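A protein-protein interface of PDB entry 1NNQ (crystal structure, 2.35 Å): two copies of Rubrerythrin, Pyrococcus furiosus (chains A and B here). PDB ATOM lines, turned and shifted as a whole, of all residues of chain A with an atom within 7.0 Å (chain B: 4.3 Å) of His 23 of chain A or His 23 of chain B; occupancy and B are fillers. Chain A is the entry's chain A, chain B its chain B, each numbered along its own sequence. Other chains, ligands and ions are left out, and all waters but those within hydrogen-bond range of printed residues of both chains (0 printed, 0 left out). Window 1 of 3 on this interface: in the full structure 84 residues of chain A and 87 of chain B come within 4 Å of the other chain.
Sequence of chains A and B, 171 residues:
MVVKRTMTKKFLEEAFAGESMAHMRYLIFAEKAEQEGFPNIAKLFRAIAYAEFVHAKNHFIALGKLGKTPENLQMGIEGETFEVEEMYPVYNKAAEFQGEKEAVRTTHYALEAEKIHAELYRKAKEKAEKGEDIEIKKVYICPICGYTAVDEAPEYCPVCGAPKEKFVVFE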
ATOM      1  N   ALA A  17     -28.589  22.253   5.596  1.00  0.00           N
ATOM      2  CA  ALA A  17     -28.448  21.598   4.317  1.00  0.00           C
ATOM      3  C   ALA A  17     -29.662  21.944   3.466  1.00  0.00           C
ATOM      4  O   ALA A  17     -29.517  22.370   2.328  1.00  0.00           O
ATOM      5  CB  ALA A  17     -28.291  20.077   4.482  1.00  0.00           C
ATOM      6  N   GLY A  18     -30.849  21.851   4.045  1.00  0.00           N
ATOM      7  CA  GLY A  18     -32.096  22.065   3.298  1.00  0.00           C
ATOM      8  C   GLY A  18     -32.200  23.469   2.737  1.00  0.00           C
ATOM      9  O   GLY A  18     -32.625  23.668   1.590  1.00  0.00           O
ATOM     10  N   GLU A  19     -31.816  24.445   3.555  1.00  0.00           N
ATOM     11  CA  GLU A  19     -31.891  25.843   3.189  1.00  0.00           C
ATOM     12  C   GLU A  19     -30.827  26.179   2.139  1.00  0.00           C
ATOM     13  O   GLU A  19     -31.061  26.978   1.224  1.00  0.00           O
ATOM     14  CB  GLU A  19     -31.717  26.730   4.426  1.00  0.00           C
ATOM     15  CG  GLU A  19     -32.847  26.629   5.431  1.00  0.00           C
ATOM     16  CD  GLU A  19     -34.101  27.369   5.012  1.00  0.00           C
ATOM     17  OE1 GLU A  19     -35.168  27.134   5.625  1.00  0.00           O
ATOM     18  OE2 GLU A  19     -34.034  28.222   4.093  1.00  0.00           O
ATOM     19  N   SER A  20     -29.654  25.568   2.281  1.00  0.00           N
ATOM     20  CA  SER A  20     -28.601  25.741   1.287  1.00  0.00           C
ATOM     21  C   SER A  20     -29.043  25.243  -0.088  1.00  0.00           C
ATOM     22  O   SER A  20     -28.869  25.932  -1.102  1.00  0.00           O
ATOM     23  CB  SER A  20     -27.335  25.028   1.727  1.00  0.00           C
ATOM     24  OG  SER A  20     -26.874  25.579   2.949  1.00  0.00           O
ATOM     25  N   MET A  21     -29.623  24.051  -0.122  1.00  0.00           N
ATOM     26  CA  MET A  21     -30.109  23.493  -1.365  1.00  0.00           C
ATOM     27  C   MET A  21     -31.179  24.352  -2.030  1.00  0.00           C
ATOM     28  O   MET A  21     -31.124  24.602  -3.237  1.00  0.00           O
ATOM     29  CB  MET A  21     -30.526  22.049  -1.153  1.00  0.00           C
ATOM     30  CG  MET A  21     -29.276  21.172  -1.038  1.00  0.00           C
ATOM     31  SD  MET A  21     -29.599  19.474  -1.183  1.00  0.00           S
ATOM     32  CE  MET A  21     -30.233  19.184   0.462  1.00  0.00           C
ATOM     33  N   ALA A  22     -32.101  24.866  -1.226  1.00  0.00           N
ATOM     34  CA  ALA A  22     -33.199  25.676  -1.728  1.00  0.00           C
ATOM     35  C   ALA A  22     -32.689  27.012  -2.275  1.00  0.00           C
ATOM     36  O   ALA A  22     -33.103  27.450  -3.354  1.00  0.00           O
ATOM     37  CB  ALA A  22     -34.246  25.885  -0.637  1.00  0.00           C
ATOM     38  N   HIS A  23     -31.782  27.641  -1.531  1.00  0.00           N
ATOM     39  CA  HIS A  23     -31.116  28.841  -1.977  1.00  0.00           C
ATOM     40  C   HIS A  23     -30.470  28.572  -3.332  1.00  0.00           C
ATOM     41  O   HIS A  23     -30.626  29.370  -4.244  1.00  0.00           O
ATOM     42  CB  HIS A  23     -30.060  29.273  -0.963  1.00  0.00           C
ATOM     43  CG  HIS A  23     -29.159  30.367  -1.449  1.00  0.00           C
ATOM     44  ND1 HIS A  23     -29.415  31.704  -1.217  1.00  0.00           N
ATOM     45  CD2 HIS A  23     -27.990  30.324  -2.133  1.00  0.00           C
ATOM     46  CE1 HIS A  23     -28.452  32.439  -1.754  1.00  0.00           C
ATOM     47  NE2 HIS A  23     -27.578  31.626  -2.319  1.00  0.00           N
ATOM     48  N   MET A  24     -29.750  27.451  -3.446  1.00  0.00           N
ATOM     49  CA  MET A  24     -29.030  27.113  -4.664  1.00  0.00           C
ATOM     50  C   MET A  24     -30.004  26.825  -5.830  1.00  0.00           C
ATOM     51  O   MET A  24     -29.826  27.326  -6.941  1.00  0.00           O
ATOM     52  CB  MET A  24     -28.112  25.911  -4.423  1.00  0.00           C
ATOM     53  CG  MET A  24     -27.266  25.555  -5.624  1.00  0.00           C
ATOM     54  SD  MET A  24     -26.154  26.858  -6.225  1.00  0.00           S
ATOM     55  CE  MET A  24     -24.862  26.839  -4.893  1.00  0.00           C
ATOM     56  N   ARG A  25     -31.035  26.033  -5.561  1.00  0.00           N
ATOM     57  CA  ARG A  25     -32.073  25.773  -6.552  1.00  0.00           C
ATOM     58  C   ARG A  25     -32.646  27.085  -7.080  1.00  0.00           C
ATOM     59  O   ARG A  25     -32.761  27.277  -8.296  1.00  0.00           O
ATOM     60  CB  ARG A  25     -33.163  24.860  -5.972  1.00  0.00           C
ATOM     61  CG  ARG A  25     -32.756  23.379  -5.965  1.00  0.00           C
ATOM     62  CD  ARG A  25     -33.899  22.380  -5.751  1.00  0.00           C
ATOM     63  NE  ARG A  25     -34.585  22.686  -4.510  1.00  0.00           N
ATOM     64  CZ  ARG A  25     -34.359  22.101  -3.333  1.00  0.00           C
ATOM     65  NH1 ARG A  25     -35.061  22.510  -2.277  1.00  0.00           N
ATOM     66  NH2 ARG A  25     -33.488  21.100  -3.222  1.00  0.00           N
ATOM     67  N   TYR A  26     -32.956  28.007  -6.172  1.00  0.00           N
ATOM     68  CA  TYR A  26     -33.552  29.281  -6.571  1.00  0.00           C
ATOM     69  C   TYR A  26     -32.643  30.170  -7.412  1.00  0.00           C
ATOM     70  O   TYR A  26     -33.128  30.871  -8.293  1.00  0.00           O
ATOM     71  CB  TYR A  26     -34.117  30.030  -5.370  1.00  0.00           C
ATOM     72  CG  TYR A  26     -35.220  29.270  -4.676  1.00  0.00           C
ATOM     73  CD1 TYR A  26     -35.537  29.525  -3.332  1.00  0.00           C
ATOM     74  CD2 TYR A  26     -35.939  28.263  -5.349  1.00  0.00           C
ATOM     75  CE1 TYR A  26     -36.544  28.787  -2.666  1.00  0.00           C
ATOM     76  CE2 TYR A  26     -36.944  27.521  -4.694  1.00  0.00           C
ATOM     77  CZ  TYR A  26     -37.237  27.797  -3.356  1.00  0.00           C
ATOM     78  OH  TYR A  26     -38.235  27.102  -2.731  1.00  0.00           O
ATOM     79  N   LEU A  27     -31.335  30.148  -7.153  1.00  0.00           N
ATOM     80  CA  LEU A  27     -30.398  30.903  -7.988  1.00  0.00           C
ATOM     81  C   LEU A  27     -30.264  30.301  -9.408  1.00  0.00           C
ATOM     82  O   LEU A  27     -30.040  31.016 -10.391  1.00  0.00           O
ATOM     83  CB  LEU A  27     -29.017  31.005  -7.333  1.00  0.00           C
ATOM     84  CG  LEU A  27     -28.790  31.746  -6.017  1.00  0.00           C
ATOM     85  CD1 LEU A  27     -27.310  31.572  -5.681  1.00  0.00           C
ATOM     86  CD2 LEU A  27     -29.137  33.256  -6.072  1.00  0.00           C
ATOM     87  N   ILE A  28     -30.373  28.985  -9.490  1.00  0.00           N
ATOM     88  CA  ILE A  28     -30.311  28.266 -10.754  1.00  0.00           C
ATOM     89  C   ILE A  28     -31.612  28.537 -11.490  1.00  0.00           C
ATOM     90  O   ILE A  28     -31.611  28.746 -12.702  1.00  0.00           O
ATOM     91  CB  ILE A  28     -30.129  26.751 -10.488  1.00  0.00           C
ATOM     92  CG1 ILE A  28     -28.736  26.484  -9.895  1.00  0.00           C
ATOM     93  CG2 ILE A  28     -30.404  25.895 -11.766  1.00  0.00           C
ATOM     94  CD1 ILE A  28     -28.595  25.082  -9.246  1.00  0.00           C
ATOM     95  N   PHE A  29     -32.717  28.558 -10.752  1.00  0.00           N
ATOM     96  CA  PHE A  29     -34.025  28.817 -11.348  1.00  0.00           C
ATOM     97  C   PHE A  29     -34.120  30.271 -11.842  1.00  0.00           C
ATOM     98  O   PHE A  29     -34.773  30.542 -12.856  1.00  0.00           O
ATOM     99  CB  PHE A  29     -35.157  28.510 -10.365  1.00  0.00           C
ATOM    100  CG  PHE A  29     -35.355  27.027 -10.074  1.00  0.00           C
ATOM    101  CD1 PHE A  29     -36.123  26.624  -8.969  1.00  0.00           C
ATOM    102  CD2 PHE A  29     -34.790  26.049 -10.890  1.00  0.00           C
ATOM    103  CE1 PHE A  29     -36.326  25.280  -8.687  1.00  0.00           C
ATOM    104  CE2 PHE A  29     -34.985  24.694 -10.617  1.00  0.00           C
ATOM    105  CZ  PHE A  29     -35.755  24.311  -9.500  1.00  0.00           C
ATOM    106  N   PHE A  45     -37.310  34.759  -7.515  1.00  0.00           N
ATOM    107  CA  PHE A  45     -36.407  33.681  -7.126  1.00  0.00           C
ATOM    108  C   PHE A  45     -35.146  34.161  -6.351  1.00  0.00           C
ATOM    109  O   PHE A  45     -34.767  33.523  -5.360  1.00  0.00           O
ATOM    110  CB  PHE A  45     -35.936  32.931  -8.370  1.00  0.00           C
ATOM    111  CG  PHE A  45     -36.839  31.827  -8.810  1.00  0.00           C
ATOM    112  CD1 PHE A  45     -37.251  30.832  -7.922  1.00  0.00           C
ATOM    113  CD2 PHE A  45     -37.270  31.765 -10.149  1.00  0.00           C
ATOM    114  CE1 PHE A  45     -38.085  29.797  -8.351  1.00  0.00           C
ATOM    115  CE2 PHE A  45     -38.082  30.727 -10.584  1.00  0.00           C
ATOM    116  CZ  PHE A  45     -38.503  29.747  -9.693  1.00  0.00           C
ATOM    117  N   ARG A  46     -34.490  35.239  -6.818  1.00  0.00           N
ATOM    118  CA  ARG A  46     -33.275  35.755  -6.156  1.00  0.00           C
ATOM    119  C   ARG A  46     -33.561  36.278  -4.746  1.00  0.00           C
ATOM    120  O   ARG A  46     -32.747  36.091  -3.823  1.00  0.00           O
ATOM    121  CB  ARG A  46     -32.563  36.878  -6.954  1.00  0.00           C
ATOM    122  CG  ARG A  46     -32.404  36.644  -8.439  1.00  0.00           C
ATOM    123  CD  ARG A  46     -31.266  37.413  -9.131  1.00  0.00           C
ATOM    124  NE  ARG A  46     -30.563  36.519 -10.068  1.00  0.00           N
ATOM    125  CZ  ARG A  46     -30.824  36.436 -11.387  1.00  0.00           C
ATOM    126  NH1 ARG A  46     -31.772  37.218 -11.932  1.00  0.00           N
ATOM    127  NH2 ARG A  46     -30.132  35.571 -12.154  1.00  0.00           N
ATOM    128  N   ILE A  48     -36.256  35.467  -2.739  1.00  0.00           N
ATOM    129  CA  ILE A  48     -36.521  34.317  -1.909  1.00  0.00           C
ATOM    130  C   ILE A  48     -35.227  33.536  -1.596  1.00  0.00           C
ATOM    131  O   ILE A  48     -35.076  33.048  -0.478  1.00  0.00           O
ATOM    132  CB  ILE A  48     -37.607  33.430  -2.513  1.00  0.00           C
ATOM    133  CG1 ILE A  48     -38.915  34.250  -2.664  1.00  0.00           C
ATOM    134  CG2 ILE A  48     -37.799  32.178  -1.643  1.00  0.00           C
ATOM    135  CD1 ILE A  48     -40.221  33.433  -2.866  1.00  0.00           C
ATOM    136  N   ALA A  49     -34.291  33.449  -2.551  1.00  0.00           N
ATOM    137  CA  ALA A  49     -32.996  32.839  -2.267  1.00  0.00           C
ATOM    138  C   ALA A  49     -32.275  33.557  -1.115  1.00  0.00           C
ATOM    139  O   ALA A  49     -31.559  32.924  -0.319  1.00  0.00           O
ATOM    140  CB  ALA A  49     -32.109  32.819  -3.508  1.00  0.00           C
ATOM    141  N   TYR A  50     -32.432  34.883  -1.058  1.00  0.00           N
ATOM    142  CA  TYR A  50     -31.820  35.645   0.015  1.00  0.00           C
ATOM    143  C   TYR A  50     -32.487  35.307   1.354  1.00  0.00           C
ATOM    144  O   TYR A  50     -31.817  35.235   2.383  1.00  0.00           O
ATOM    145  CB  TYR A  50     -31.834  37.156  -0.254  1.00  0.00           C
ATOM    146  CG  TYR A  50     -31.222  37.958   0.886  1.00  0.00           C
ATOM    147  CD1 TYR A  50     -29.856  37.947   1.119  1.00  0.00           C
ATOM    148  CD2 TYR A  50     -32.022  38.722   1.732  1.00  0.00           C
ATOM    149  CE1 TYR A  50     -29.300  38.695   2.175  1.00  0.00           C
ATOM    150  CE2 TYR A  50     -31.490  39.446   2.785  1.00  0.00           C
ATOM    151  CZ  TYR A  50     -30.142  39.430   3.001  1.00  0.00           C
ATOM    152  OH  TYR A  50     -29.628  40.157   4.049  1.00  0.00           O
ATOM    153  N   ALA A  51     -33.801  35.095   1.333  1.00  0.00           N
ATOM    154  CA  ALA A  51     -34.523  34.672   2.530  1.00  0.00           C
ATOM    155  C   ALA A  51     -33.998  33.321   3.036  1.00  0.00           C
ATOM    156  O   ALA A  51     -33.800  33.167   4.231  1.00  0.00           O
ATOM    157  CB  ALA A  51     -36.019  34.610   2.276  1.00  0.00           C
ATOM    158  N   GLU A  52     -33.782  32.358   2.138  1.00  0.00           N
ATOM    159  CA  GLU A  52     -33.198  31.069   2.503  1.00  0.00           C
ATOM    160  C   GLU A  52     -31.784  31.216   3.099  1.00  0.00           C
ATOM    161  O   GLU A  52     -31.427  30.482   4.019  1.00  0.00           O
ATOM    162  CB  GLU A  52     -33.188  30.095   1.305  1.00  0.00           C
ATOM    163  CG  GLU A  52     -34.481  29.998   0.459  1.00  0.00           C
ATOM    164  CD  GLU A  52     -35.772  29.728   1.236  1.00  0.00           C
ATOM    165  OE1 GLU A  52     -36.826  29.466   0.620  1.00  0.00           O
ATOM    166  OE2 GLU A  52     -35.789  29.803   2.470  1.00  0.00           O
ATOM    167  N   PHE A  53     -30.988  32.142   2.554  1.00  0.00           N
ATOM    168  CA  PHE A  53     -29.673  32.498   3.081  1.00  0.00           C
ATOM    169  C   PHE A  53     -29.804  32.986   4.525  1.00  0.00           C
ATOM    170  O   PHE A  53     -29.001  32.608   5.382  1.00  0.00           O
ATOM    171  CB  PHE A  53     -29.013  33.612   2.226  1.00  0.00           C
ATOM    172  CG  PHE A  53     -27.916  34.374   2.951  1.00  0.00           C
ATOM    173  CD1 PHE A  53     -26.628  33.856   3.023  1.00  0.00           C
ATOM    174  CD2 PHE A  53     -28.188  35.591   3.577  1.00  0.00           C
ATOM    175  CE1 PHE A  53     -25.625  34.534   3.711  1.00  0.00           C
ATOM    176  CE2 PHE A  53     -27.197  36.293   4.258  1.00  0.00           C
ATOM    177  CZ  PHE A  53     -25.912  35.758   4.330  1.00  0.00           C
ATOM    178  N   VAL A  54     -30.798  33.851   4.779  1.00  0.00           N
ATOM    179  CA  VAL A  54     -31.054  34.356   6.128  1.00  0.00           C
ATOM    180  C   VAL A  54     -31.342  33.174   7.048  1.00  0.00           C
ATOM    181  O   VAL A  54     -30.698  33.017   8.095  1.00  0.00           O
ATOM    182  CB  VAL A  54     -32.217  35.403   6.163  1.00  0.00           C
ATOM    183  CG1 VAL A  54     -32.576  35.786   7.618  1.00  0.00           C
ATOM    184  CG2 VAL A  54     -31.829  36.683   5.364  1.00  0.00           C
ATOM    185  N   ALA A  56     -30.577  29.953   6.661  1.00  0.00           N
ATOM    186  CA  ALA A  56     -29.410  29.091   6.798  1.00  0.00           C
ATOM    187  C   ALA A  56     -28.380  29.717   7.749  1.00  0.00           C
ATOM    188  O   ALA A  56     -27.805  29.020   8.581  1.00  0.00           O
ATOM    189  CB  ALA A  56     -28.772  28.778   5.412  1.00  0.00           C
ATOM    190  N   GLU B  19     -22.036  21.078  -2.375  1.00  0.00           N
ATOM    191  CA  GLU B  19     -21.690  22.302  -3.099  1.00  0.00           C
ATOM    192  C   GLU B  19     -22.552  23.467  -2.621  1.00  0.00           C
ATOM    193  O   GLU B  19     -22.064  24.608  -2.498  1.00  0.00           O
ATOM    194  CB  GLU B  19     -21.853  22.141  -4.625  1.00  0.00           C
ATOM    195  CG  GLU B  19     -20.867  21.207  -5.295  1.00  0.00           C
ATOM    196  CD  GLU B  19     -19.447  21.744  -5.291  1.00  0.00           C
ATOM    197  OE1 GLU B  19     -19.253  22.954  -4.994  1.00  0.00           O
ATOM    198  OE2 GLU B  19     -18.514  20.979  -5.617  1.00  0.00           O
ATOM    199  N   SER B  20     -23.834  23.168  -2.374  1.00  0.00           N
ATOM    200  CA  SER B  20     -24.795  24.131  -1.865  1.00  0.00           C
ATOM    201  C   SER B  20     -24.390  24.648  -0.487  1.00  0.00           C
ATOM    202  O   SER B  20     -24.424  25.848  -0.237  1.00  0.00           O
ATOM    203  CB  SER B  20     -26.180  23.503  -1.797  1.00  0.00           C
ATOM    204  OG  SER B  20     -26.583  23.073  -3.085  1.00  0.00           O
ATOM    205  N   MET B  21     -23.987  23.746   0.401  1.00  0.00           N
ATOM    206  CA  MET B  21     -23.548  24.139   1.744  1.00  0.00           C
ATOM    207  C   MET B  21     -22.250  24.940   1.732  1.00  0.00           C
ATOM    208  O   MET B  21     -22.106  25.904   2.490  1.00  0.00           O
ATOM    209  CB  MET B  21     -23.435  22.917   2.646  1.00  0.00           C
ATOM    210  CG  MET B  21     -24.808  22.383   3.025  1.00  0.00           C
ATOM    211  SD  MET B  21     -24.747  21.100   4.300  1.00  0.00           S
ATOM    212  CE  MET B  21     -24.394  19.745   3.256  1.00  0.00           C
ATOM    213  N   ALA B  22     -21.329  24.567   0.849  1.00  0.00           N
ATOM    214  CA  ALA B  22     -20.058  25.266   0.738  1.00  0.00           C
ATOM    215  C   ALA B  22     -20.285  26.693   0.252  1.00  0.00           C
ATOM    216  O   ALA B  22     -19.715  27.620   0.787  1.00  0.00           O
ATOM    217  CB  ALA B  22     -19.080  24.517  -0.172  1.00  0.00           C
ATOM    218  N   HIS B  23     -21.146  26.846  -0.749  1.00  0.00           N
ATOM    219  CA  HIS B  23     -21.553  28.141  -1.263  1.00  0.00           C
ATOM    220  C   HIS B  23     -22.169  28.992  -0.169  1.00  0.00           C
ATOM    221  O   HIS B  23     -21.840  30.176  -0.039  1.00  0.00           O
ATOM    222  CB  HIS B  23     -22.575  27.931  -2.393  1.00  0.00           C
ATOM    223  CG  HIS B  23     -23.300  29.170  -2.803  1.00  0.00           C
ATOM    224  ND1 HIS B  23     -22.871  29.977  -3.839  1.00  0.00           N
ATOM    225  CD2 HIS B  23     -24.456  29.711  -2.357  1.00  0.00           C
ATOM    226  CE1 HIS B  23     -23.726  30.973  -3.996  1.00  0.00           C
ATOM    227  NE2 HIS B  23     -24.704  30.827  -3.120  1.00  0.00           N
ATOM    228  N   MET B  24     -23.084  28.383   0.587  1.00  0.00           N
ATOM    229  CA  MET B  24     -23.766  29.047   1.683  1.00  0.00           C
ATOM    230  C   MET B  24     -22.772  29.508   2.775  1.00  0.00           C
ATOM    231  O   MET B  24     -22.761  30.678   3.166  1.00  0.00           O
ATOM    232  CB  MET B  24     -24.841  28.137   2.256  1.00  0.00           C
ATOM    233  CG  MET B  24     -25.704  28.794   3.301  1.00  0.00           C
ATOM    234  SD  MET B  24     -26.523  30.316   2.719  1.00  0.00           S
ATOM    235  CE  MET B  24     -27.892  29.605   1.675  1.00  0.00           C
ATOM    236  N   ARG B  25     -21.926  28.585   3.222  1.00  0.00           N
ATOM    237  CA  ARG B  25     -20.852  28.868   4.179  1.00  0.00           C
ATOM    238  C   ARG B  25     -19.977  30.023   3.702  1.00  0.00           C
ATOM    239  O   ARG B  25     -19.680  30.953   4.470  1.00  0.00           O
ATOM    240  CB  ARG B  25     -20.011  27.613   4.429  1.00  0.00           C
ATOM    241  CG  ARG B  25     -20.653  26.658   5.421  1.00  0.00           C
ATOM    242  CD  ARG B  25     -19.691  25.603   6.020  1.00  0.00           C
ATOM    243  NE  ARG B  25     -19.103  24.848   4.926  1.00  0.00           N
ATOM    244  CZ  ARG B  25     -19.558  23.689   4.472  1.00  0.00           C
ATOM    245  NH1 ARG B  25     -18.947  23.145   3.442  1.00  0.00           N
ATOM    246  NH2 ARG B  25     -20.570  23.060   5.069  1.00  0.00           N
ATOM    247  N   TYR B  26     -19.586  29.999   2.430  1.00  0.00           N
ATOM    248  CA  TYR B  26     -18.733  31.078   1.909  1.00  0.00           C
ATOM    249  C   TYR B  26     -19.440  32.447   1.876  1.00  0.00           C
ATOM    250  O   TYR B  26     -18.812  33.478   2.110  1.00  0.00           O
ATOM    251  CB  TYR B  26     -18.131  30.706   0.552  1.00  0.00           C
ATOM    252  CG  TYR B  26     -17.213  29.496   0.627  1.00  0.00           C
ATOM    253  CD1 TYR B  26     -16.955  28.715  -0.504  1.00  0.00           C
ATOM    254  CD2 TYR B  26     -16.631  29.117   1.844  1.00  0.00           C
ATOM    255  CE1 TYR B  26     -16.105  27.578  -0.438  1.00  0.00           C
ATOM    256  CE2 TYR B  26     -15.806  27.994   1.933  1.00  0.00           C
ATOM    257  CZ  TYR B  26     -15.539  27.229   0.791  1.00  0.00           C
ATOM    258  OH  TYR B  26     -14.704  26.149   0.909  1.00  0.00           O
ATOM    259  N   LEU B  27     -20.742  32.451   1.622  1.00  0.00           N
ATOM    260  CA  LEU B  27     -21.509  33.687   1.664  1.00  0.00           C
ATOM    261  C   LEU B  27     -21.609  34.221   3.107  1.00  0.00           C
ATOM    262  O   LEU B  27     -21.553  35.424   3.324  1.00  0.00           O
ATOM    263  CB  LEU B  27     -22.904  33.503   1.049  1.00  0.00           C
ATOM    264  CG  LEU B  27     -23.107  33.281  -0.466  1.00  0.00           C
ATOM    265  CD1 LEU B  27     -24.598  33.268  -0.801  1.00  0.00           C
ATOM    266  CD2 LEU B  27     -22.414  34.366  -1.317  1.00  0.00           C
ATOM    267  N   ALA B  49     -17.565  31.204  -3.775  1.00  0.00           N
ATOM    268  CA  ALA B  49     -18.967  30.835  -3.605  1.00  0.00           C
ATOM    269  C   ALA B  49     -19.647  30.712  -4.961  1.00  0.00           C
ATOM    270  O   ALA B  49     -20.433  29.788  -5.180  1.00  0.00           O
ATOM    271  CB  ALA B  49     -19.720  31.865  -2.730  1.00  0.00           C
ATOM    272  N   GLU B  52     -18.619  27.469  -6.551  1.00  0.00           N
ATOM    273  CA  GLU B  52     -19.438  26.390  -6.012  1.00  0.00           C
ATOM    274  C   GLU B  52     -20.844  26.374  -6.650  1.00  0.00           C
ATOM    275  O   GLU B  52     -21.398  25.322  -6.912  1.00  0.00           O
ATOM    276  CB  GLU B  52     -19.525  26.462  -4.476  1.00  0.00           C
ATOM    277  CG  GLU B  52     -18.219  26.774  -3.715  1.00  0.00           C
ATOM    278  CD  GLU B  52     -17.029  25.865  -4.026  1.00  0.00           C
ATOM    279  OE1 GLU B  52     -16.994  25.140  -5.032  1.00  0.00           O
ATOM    280  OE2 GLU B  52     -16.056  25.898  -3.276  1.00  0.00           O
ATOM    281  N   PHE B  53     -21.404  27.549  -6.913  1.00  0.00           N
ATOM    282  CA  PHE B  53     -22.657  27.657  -7.647  1.00  0.00           C
ATOM    283  C   PHE B  53     -22.535  27.013  -9.045  1.00  0.00           C
ATOM    284  O   PHE B  53     -23.450  26.328  -9.488  1.00  0.00           O
ATOM    285  CB  PHE B  53     -23.143  29.117  -7.748  1.00  0.00           C
ATOM    286  CG  PHE B  53     -24.092  29.357  -8.913  1.00  0.00           C
ATOM    287  CD1 PHE B  53     -25.460  29.204  -8.750  1.00  0.00           C
ATOM    288  CD2 PHE B  53     -23.599  29.700 -10.182  1.00  0.00           C
ATOM    289  CE1 PHE B  53     -26.337  29.402  -9.832  1.00  0.00           C
ATOM    290  CE2 PHE B  53     -24.451  29.905 -11.274  1.00  0.00           C
ATOM    291  CZ  PHE B  53     -25.829  29.756 -11.103  1.00  0.00           C
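A ring nitrogen (NE2) of His 23 of chain A sits at hydrogen-bond distance from a ring nitrogen (NE2) of His 23 of chain B, at 3.1 Å.
ND1 of His 23 of chain A is in hydrogen-bond range of O of Ala 49 of chain A.
A ring nitrogen (ND1) of His 23 of chain B is in hydrogen-bond range of the backbone carbonyl oxygen (O) of Ala 49 of chain B (2.8 Å).
Among the printed residues, merely in contact across the chains: Ser 20 of chain A with Met 24 of chain B, His 23 of chain A with Met 24 of chain B, Met 24 of chain A with Ser 20 of chain B, Met 24 of chain A with His 23 of chain B, Met 24 of chain A with Phe 53 of chain B, Phe 53 of chain A with Met 24 of chain B, Ser 20 of chain A with Ser 20 of chain B, Ala 17 of chain A with Met 21 of chain B, Ala 56 of chain A with Met 24 of chain B, His 23 of chain A with Leu 27 of chain B, Leu 27 of chain A with His 23 of chain B, Ile 28 of chain A with Phe 53 of chain B, Ser 20 of chain A with Met 21 of chain B, Met 21 of chain A with Ser 20 of chain B, Phe 53 of chain A with Leu 27 of chain B and Leu 27 of chain A with Phe 53 of chain B.
Ala 22 of chain A touches none of the printed residues of chain B.
Of chain B, only His 23 (3.1 Å), Met 24 (3.4 Å) and Leu 27 (3.7 Å) come within 4 Å of His 23 of chain A.
Of chain A, only His 23 (3.1 Å), Met 24 (3.5 Å) and Leu 27 (3.7 Å) come within 4 Å of His 23 of chain B.
Of the printed residues of chain A, Met 24 of chain B touches Ser 20 (3.3 Å), His 23 (3.4 Å), Phe 53 (3.6 Å) and Ala 56 (3.7 Å).
Printed residues of chain A within 4 Å of Leu 27 of chain B: His 23 (3.7 Å) and Phe 53 (3.9 Å).
The nearest residue of chain A that does not touch His 23 of chain B is Ser 20 of chain A (5.9 Å).
Printed residues of chain A that touch a printed residue of chain B: Ala 17, Ser 20, Met 21, His 23, Met 24, Leu 27, Ile 28, Phe 53 and Ala 56.
Hydrophobic or aromatic side chains of chain B within 4 Å of the printed part of chain A: Met 21, His 23, Met 24, Leu 27 and Phe 53.
Among the printed residues, no Asp or Glu carboxylate lies within 4 Å of a Lys or Arg side-chain nitrogen of the other chain.
Ser 20 of chain A touches Met 21 of chain B, and with the chains exchanged Met 21 of chain A touches Ser 20 of chain B.
Ser 20 of chain A touches Met 24 of chain B, and with the chains exchanged Met 24 of chain A touches Ser 20 of chain B.
His 23 of chain A touches Met 24 of chain B, and with the chains exchanged Met 24 of chain A touches His 23 of chain B.
His 23 of chain A touches Leu 27 of chain B, and with the chains exchanged Leu 27 of chain A touches His 23 of chain B.
12 positions are printed for both chains.
Of the 17 pairs that touch across the chains among the printed residues, 14 have their exchanged pair printed and touching as well.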
